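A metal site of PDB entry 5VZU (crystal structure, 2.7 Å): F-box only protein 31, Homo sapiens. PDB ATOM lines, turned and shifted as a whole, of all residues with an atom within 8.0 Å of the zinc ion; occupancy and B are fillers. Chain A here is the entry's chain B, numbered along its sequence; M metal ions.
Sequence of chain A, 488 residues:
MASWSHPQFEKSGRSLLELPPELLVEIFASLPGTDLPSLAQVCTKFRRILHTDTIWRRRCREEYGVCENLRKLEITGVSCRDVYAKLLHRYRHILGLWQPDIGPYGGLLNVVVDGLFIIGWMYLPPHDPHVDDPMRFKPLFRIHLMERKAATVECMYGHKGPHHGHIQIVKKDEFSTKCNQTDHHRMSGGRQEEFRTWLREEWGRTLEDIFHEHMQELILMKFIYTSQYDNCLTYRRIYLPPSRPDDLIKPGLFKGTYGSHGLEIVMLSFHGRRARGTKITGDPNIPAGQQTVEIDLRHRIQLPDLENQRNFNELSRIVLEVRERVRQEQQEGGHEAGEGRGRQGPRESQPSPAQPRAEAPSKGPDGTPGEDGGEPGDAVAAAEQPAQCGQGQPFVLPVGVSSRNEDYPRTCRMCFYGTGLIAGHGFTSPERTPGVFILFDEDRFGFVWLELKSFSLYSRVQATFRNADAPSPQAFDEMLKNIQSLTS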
ATOM      1  N   LEU A 140     -23.940  26.492  -3.577  1.00  0.00           N
ATOM      2  CA  LEU A 140     -23.385  27.339  -4.608  1.00  0.00           C
ATOM      3  C   LEU A 140     -21.882  27.289  -4.699  1.00  0.00           C
ATOM      4  O   LEU A 140     -21.333  27.336  -5.799  1.00  0.00           O
ATOM      5  CB  LEU A 140     -23.756  28.789  -4.378  1.00  0.00           C
ATOM      6  CG  LEU A 140     -24.958  29.315  -5.117  1.00  0.00           C
ATOM      7  CD1 LEU A 140     -24.973  30.831  -4.951  1.00  0.00           C
ATOM      8  CD2 LEU A 140     -24.918  28.929  -6.585  1.00  0.00           C
ATOM      9  N   GLU A 154     -14.166  26.076  -4.442  1.00  0.00           N
ATOM     10  CA  GLU A 154     -14.782  25.514  -5.626  1.00  0.00           C
ATOM     11  C   GLU A 154     -16.185  26.088  -5.856  1.00  0.00           C
ATOM     12  O   GLU A 154     -16.955  26.264  -4.932  1.00  0.00           O
ATOM     13  CB  GLU A 154     -14.861  24.005  -5.527  1.00  0.00           C
ATOM     14  CG  GLU A 154     -13.540  23.256  -5.396  1.00  0.00           C
ATOM     15  CD  GLU A 154     -13.741  21.906  -4.695  1.00  0.00           C
ATOM     16  OE1 GLU A 154     -13.957  21.922  -3.472  1.00  0.00           O
ATOM     17  OE2 GLU A 154     -13.751  20.853  -5.353  1.00  0.00           O
ATOM     18  N   CYS A 155     -16.528  26.371  -7.101  1.00  0.00           N
ATOM     19  CA  CYS A 155     -17.887  26.748  -7.466  1.00  0.00           C
ATOM     20  C   CYS A 155     -18.691  25.465  -7.677  1.00  0.00           C
ATOM     21  O   CYS A 155     -18.225  24.577  -8.381  1.00  0.00           O
ATOM     22  CB  CYS A 155     -17.891  27.571  -8.752  1.00  0.00           C
ATOM     23  SG  CYS A 155     -19.520  27.964  -9.385  1.00  0.00           S
ATOM     24  N   MET A 156     -19.883  25.391  -7.104  1.00  0.00           N
ATOM     25  CA  MET A 156     -20.765  24.203  -7.170  1.00  0.00           C
ATOM     26  C   MET A 156     -21.961  24.378  -8.110  1.00  0.00           C
ATOM     27  O   MET A 156     -22.878  23.575  -8.144  1.00  0.00           O
ATOM     28  CB  MET A 156     -21.295  23.928  -5.775  1.00  0.00           C
ATOM     29  CG  MET A 156     -20.181  23.713  -4.780  1.00  0.00           C
ATOM     30  SD  MET A 156     -19.517  22.069  -5.027  1.00  0.00           S
ATOM     31  CE  MET A 156     -20.889  21.125  -4.343  1.00  0.00           C
ATOM     32  N   TYR A 157     -21.959  25.447  -8.867  1.00  0.00           N
ATOM     33  CA  TYR A 157     -23.078  25.746  -9.694  1.00  0.00           C
ATOM     34  C   TYR A 157     -22.909  24.918 -10.938  1.00  0.00           C
ATOM     35  O   TYR A 157     -21.800  24.744 -11.412  1.00  0.00           O
ATOM     36  CB  TYR A 157     -23.048  27.223 -10.037  1.00  0.00           C
ATOM     37  CG  TYR A 157     -24.262  27.735 -10.754  1.00  0.00           C
ATOM     38  CD1 TYR A 157     -25.528  27.633 -10.179  1.00  0.00           C
ATOM     39  CD2 TYR A 157     -24.142  28.375 -11.985  1.00  0.00           C
ATOM     40  CE1 TYR A 157     -26.646  28.130 -10.838  1.00  0.00           C
ATOM     41  CE2 TYR A 157     -25.255  28.882 -12.634  1.00  0.00           C
ATOM     42  CZ  TYR A 157     -26.489  28.749 -12.062  1.00  0.00           C
ATOM     43  OH  TYR A 157     -27.585  29.240 -12.703  1.00  0.00           O
ATOM     44  N   GLY A 158     -24.027  24.435 -11.462  1.00  0.00           N
ATOM     45  CA  GLY A 158     -24.048  23.742 -12.729  1.00  0.00           C
ATOM     46  C   GLY A 158     -24.501  22.331 -12.474  1.00  0.00           C
ATOM     47  O   GLY A 158     -24.920  22.009 -11.364  1.00  0.00           O
ATOM     48  N   GLY A 161     -20.636  19.062 -11.749  1.00  0.00           N
ATOM     49  CA  GLY A 161     -19.782  18.867 -10.578  1.00  0.00           C
ATOM     50  C   GLY A 161     -18.933  20.046 -10.124  1.00  0.00           C
ATOM     51  O   GLY A 161     -18.819  21.075 -10.813  1.00  0.00           O
ATOM     52  N   PRO A 162     -18.303  19.905  -8.937  1.00  0.00           N
ATOM     53  CA  PRO A 162     -17.378  20.892  -8.359  1.00  0.00           C
ATOM     54  C   PRO A 162     -16.228  21.269  -9.279  1.00  0.00           C
ATOM     55  O   PRO A 162     -15.704  20.386  -9.961  1.00  0.00           O
ATOM     56  CB  PRO A 162     -16.816  20.165  -7.124  1.00  0.00           C
ATOM     57  CG  PRO A 162     -17.802  19.097  -6.788  1.00  0.00           C
ATOM     58  CD  PRO A 162     -18.429  18.695  -8.092  1.00  0.00           C
ATOM     59  N   HIS A 163     -15.855  22.552  -9.302  1.00  0.00           N
ATOM     60  CA  HIS A 163     -14.777  23.098 -10.152  1.00  0.00           C
ATOM     61  C   HIS A 163     -14.242  24.412  -9.593  1.00  0.00           C
ATOM     62  O   HIS A 163     -14.712  24.902  -8.569  1.00  0.00           O
ATOM     63  CB  HIS A 163     -15.263  23.303 -11.576  1.00  0.00           C
ATOM     64  CG  HIS A 163     -16.511  24.096 -11.659  1.00  0.00           C
ATOM     65  ND1 HIS A 163     -17.737  23.589 -11.286  1.00  0.00           N
ATOM     66  CD2 HIS A 163     -16.738  25.366 -12.054  1.00  0.00           C
ATOM     67  CE1 HIS A 163     -18.664  24.510 -11.462  1.00  0.00           C
ATOM     68  NE2 HIS A 163     -18.083  25.590 -11.935  1.00  0.00           N
ATOM     69  N   HIS A 164     -13.264  25.010 -10.271  1.00  0.00           N
ATOM     70  CA  HIS A 164     -12.487  26.034  -9.605  1.00  0.00           C
ATOM     71  C   HIS A 164     -13.255  27.350  -9.474  1.00  0.00           C
ATOM     72  O   HIS A 164     -13.859  27.827 -10.413  1.00  0.00           O
ATOM     73  CB  HIS A 164     -11.111  26.207 -10.269  1.00  0.00           C
ATOM     74  CG  HIS A 164     -10.095  26.859  -9.379  1.00  0.00           C
ATOM     75  ND1 HIS A 164      -9.419  28.017  -9.718  1.00  0.00           N
ATOM     76  CD2 HIS A 164      -9.669  26.538  -8.132  1.00  0.00           C
ATOM     77  CE1 HIS A 164      -8.612  28.367  -8.739  1.00  0.00           C
ATOM     78  NE2 HIS A 164      -8.750  27.483  -7.762  1.00  0.00           N
ATOM     79  N   GLY A 165     -13.212  27.913  -8.272  1.00  0.00           N
ATOM     80  CA  GLY A 165     -13.725  29.244  -8.005  1.00  0.00           C
ATOM     81  C   GLY A 165     -12.797  30.121  -7.168  1.00  0.00           C
ATOM     82  O   GLY A 165     -11.716  29.685  -6.731  1.00  0.00           O
ATOM     83  N   LYS A 178     -16.306  34.395  -7.693  1.00  0.00           N
ATOM     84  CA  LYS A 178     -16.100  34.297  -9.121  1.00  0.00           C
ATOM     85  C   LYS A 178     -16.028  32.818  -9.460  1.00  0.00           C
ATOM     86  O   LYS A 178     -15.506  32.033  -8.681  1.00  0.00           O
ATOM     87  CB  LYS A 178     -14.791  34.996  -9.528  1.00  0.00           C
ATOM     88  CG  LYS A 178     -14.938  36.479  -9.766  1.00  0.00           C
ATOM     89  CD  LYS A 178     -13.705  37.046 -10.446  1.00  0.00           C
ATOM     90  CE  LYS A 178     -13.715  36.809 -11.957  1.00  0.00           C
ATOM     91  NZ  LYS A 178     -12.468  37.312 -12.595  1.00  0.00           N
ATOM     92  N   CYS A 179     -16.587  32.441 -10.613  1.00  0.00           N
ATOM     93  CA  CYS A 179     -16.398  31.083 -11.127  1.00  0.00           C
ATOM     94  C   CYS A 179     -15.483  31.171 -12.310  1.00  0.00           C
ATOM     95  O   CYS A 179     -15.589  32.107 -13.064  1.00  0.00           O
ATOM     96  CB  CYS A 179     -17.698  30.431 -11.524  1.00  0.00           C
ATOM     97  SG  CYS A 179     -17.414  28.996 -12.551  1.00  0.00           S
ATOM     98  N   ASN A 180     -14.569  30.219 -12.444  1.00  0.00           N
ATOM     99  CA  ASN A 180     -13.460  30.355 -13.373  1.00  0.00           C
ATOM    100  C   ASN A 180     -13.500  29.375 -14.507  1.00  0.00           C
ATOM    101  O   ASN A 180     -12.620  29.381 -15.377  1.00  0.00           O
ATOM    102  CB  ASN A 180     -12.156  30.211 -12.601  1.00  0.00           C
ATOM    103  CG  ASN A 180     -11.778  31.478 -11.886  1.00  0.00           C
ATOM    104  OD1 ASN A 180     -11.443  31.468 -10.687  1.00  0.00           O
ATOM    105  ND2 ASN A 180     -11.869  32.604 -12.604  1.00  0.00           N
ATOM    106  N   GLN A 181     -14.514  28.524 -14.506  1.00  0.00           N
ATOM    107  CA  GLN A 181     -14.643  27.524 -15.515  1.00  0.00           C
ATOM    108  C   GLN A 181     -16.119  27.399 -15.780  1.00  0.00           C
ATOM    109  O   GLN A 181     -16.727  26.385 -15.460  1.00  0.00           O
ATOM    110  CB  GLN A 181     -14.018  26.198 -15.009  1.00  0.00           C
ATOM    111  CG  GLN A 181     -12.611  26.351 -14.412  1.00  0.00           C
ATOM    112  CD  GLN A 181     -11.897  25.039 -14.192  1.00  0.00           C
ATOM    113  OE1 GLN A 181     -10.719  24.938 -14.468  1.00  0.00           O
ATOM    114  NE2 GLN A 181     -12.594  24.043 -13.688  1.00  0.00           N
ATOM    115  N   THR A 182     -16.709  28.450 -16.365  1.00  0.00           N
ATOM    116  CA  THR A 182     -18.163  28.478 -16.522  1.00  0.00           C
ATOM    117  C   THR A 182     -18.698  27.410 -17.441  1.00  0.00           C
ATOM    118  O   THR A 182     -19.893  27.068 -17.387  1.00  0.00           O
ATOM    119  CB  THR A 182     -18.681  29.833 -17.014  1.00  0.00           C
ATOM    120  OG1 THR A 182     -18.016  30.199 -18.241  1.00  0.00           O
ATOM    121  CG2 THR A 182     -18.474  30.888 -15.948  1.00  0.00           C
ATOM    122  N   ASP A 183     -17.823  26.899 -18.306  1.00  0.00           N
ATOM    123  CA  ASP A 183     -18.125  25.733 -19.130  1.00  0.00           C
ATOM    124  C   ASP A 183     -18.944  24.692 -18.343  1.00  0.00           C
ATOM    125  O   ASP A 183     -19.740  23.959 -18.925  1.00  0.00           O
ATOM    126  CB  ASP A 183     -16.850  25.129 -19.740  1.00  0.00           C
ATOM    127  CG  ASP A 183     -15.616  25.155 -18.788  1.00  0.00           C
ATOM    128  OD1 ASP A 183     -15.207  24.070 -18.288  1.00  0.00           O
ATOM    129  OD2 ASP A 183     -15.045  26.251 -18.564  1.00  0.00           O
ATOM    130  N   HIS A 184     -18.789  24.647 -17.037  1.00  0.00           N
ATOM    131  CA  HIS A 184     -19.538  23.680 -16.234  1.00  0.00           C
ATOM    132  C   HIS A 184     -21.014  23.996 -16.053  1.00  0.00           C
ATOM    133  O   HIS A 184     -21.823  23.088 -15.762  1.00  0.00           O
ATOM    134  CB  HIS A 184     -18.865  23.513 -14.869  1.00  0.00           C
ATOM    135  CG  HIS A 184     -17.536  22.815 -14.925  1.00  0.00           C
ATOM    136  ND1 HIS A 184     -16.411  23.399 -15.481  1.00  0.00           N
ATOM    137  CD2 HIS A 184     -17.149  21.593 -14.484  1.00  0.00           C
ATOM    138  CE1 HIS A 184     -15.397  22.569 -15.373  1.00  0.00           C
ATOM    139  NE2 HIS A 184     -15.809  21.470 -14.760  1.00  0.00           N
ATOM    140  N   HIS A 185     -21.394  25.269 -16.205  1.00  0.00           N
ATOM    141  CA  HIS A 185     -22.807  25.656 -16.057  1.00  0.00           C
ATOM    142  C   HIS A 185     -23.602  25.336 -17.303  1.00  0.00           C
ATOM    143  O   HIS A 185     -24.829  25.302 -17.244  1.00  0.00           O
ATOM    144  CB  HIS A 185     -23.009  27.133 -15.741  1.00  0.00           C
ATOM    145  CG  HIS A 185     -22.086  27.652 -14.707  1.00  0.00           C
ATOM    146  ND1 HIS A 185     -21.749  28.980 -14.617  1.00  0.00           N
ATOM    147  CD2 HIS A 185     -21.384  27.019 -13.741  1.00  0.00           C
ATOM    148  CE1 HIS A 185     -20.886  29.153 -13.634  1.00  0.00           C
ATOM    149  NE2 HIS A 185     -20.651  27.981 -13.094  1.00  0.00           N
ATOM    150  N   ASP A 230     -23.687  34.206 -14.105  1.00  0.00           N
ATOM    151  CA  ASP A 230     -22.826  32.999 -14.124  1.00  0.00           C
ATOM    152  C   ASP A 230     -22.166  32.762 -12.763  1.00  0.00           C
ATOM    153  O   ASP A 230     -20.974  32.447 -12.733  1.00  0.00           O
ATOM    154  CB  ASP A 230     -21.716  33.120 -15.184  1.00  0.00           C
ATOM    155  CG  ASP A 230     -21.891  32.176 -16.403  1.00  0.00           C
ATOM    156  OD1 ASP A 230     -22.700  31.198 -16.361  1.00  0.00           O
ATOM    157  OD2 ASP A 230     -21.170  32.419 -17.418  1.00  0.00           O
ATOM    158  N   ASN A 231     -22.934  32.946 -11.658  1.00  0.00           N
ATOM    159  CA  ASN A 231     -22.482  32.795 -10.234  1.00  0.00           C
ATOM    160  C   ASN A 231     -21.285  33.657  -9.786  1.00  0.00           C
ATOM    161  O   ASN A 231     -20.556  33.290  -8.820  1.00  0.00           O
ATOM    162  CB  ASN A 231     -22.195  31.350  -9.906  1.00  0.00           C
ATOM    163  CG  ASN A 231     -21.954  31.125  -8.437  1.00  0.00           C
ATOM    164  OD1 ASN A 231     -22.853  31.340  -7.641  1.00  0.00           O
ATOM    165  ND2 ASN A 231     -20.720  30.727  -8.075  1.00  0.00           N
ATOM    166  N   CYS A 232     -21.077  34.758 -10.513  1.00  0.00           N
ATOM    167  CA  CYS A 232     -20.114  35.804 -10.146  1.00  0.00           C
ATOM    168  C   CYS A 232     -20.980  36.856  -9.530  1.00  0.00           C
ATOM    169  O   CYS A 232     -21.671  37.588 -10.231  1.00  0.00           O
ATOM    170  CB  CYS A 232     -19.352  36.281 -11.323  1.00  0.00           C
ATOM    171  SG  CYS A 232     -18.763  34.815 -12.199  1.00  0.00           S
HETATM  172 ZN    ZN M   1     -19.019  27.619 -11.595  1.00  0.00          ZN
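OD1 of Asp 230 lies within hydrogen-bond range of ND1 of His 185 (3.0 Å). O of Gly 161 sits at hydrogen-bond distance from ND1 of His 163, 2.8 Å away. N of Tyr 157 lies close to SG of Cys 155. SG of Cys 155 sits close to ND2 of Asn 231. SG of Cys 179 lies close to N of Gln 181, at 3.5 Å. N of Cys 179 sits at hydrogen-bond distance from SG of Cys 232 (3.6 Å).
Within 4 Å of the zinc ion: Cys 155, His 163, Cys 179 and His 185. The nearest printed residue that does not touch the zinc ion is Tyr 157 (4.004 Å).
The zinc ion is bound by a ring nitrogen (NE2) of His 185, at 2.2 Å. A ring nitrogen (NE2) of His 163 is bound to the zinc ion (2.3 Å). The zinc ion is bound by the side-chain sulfur (SG) of Cys 155 (2.3 Å). The zinc ion is bound by SG of Cys 179. The zinc ion has four donor atoms within binding distance.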
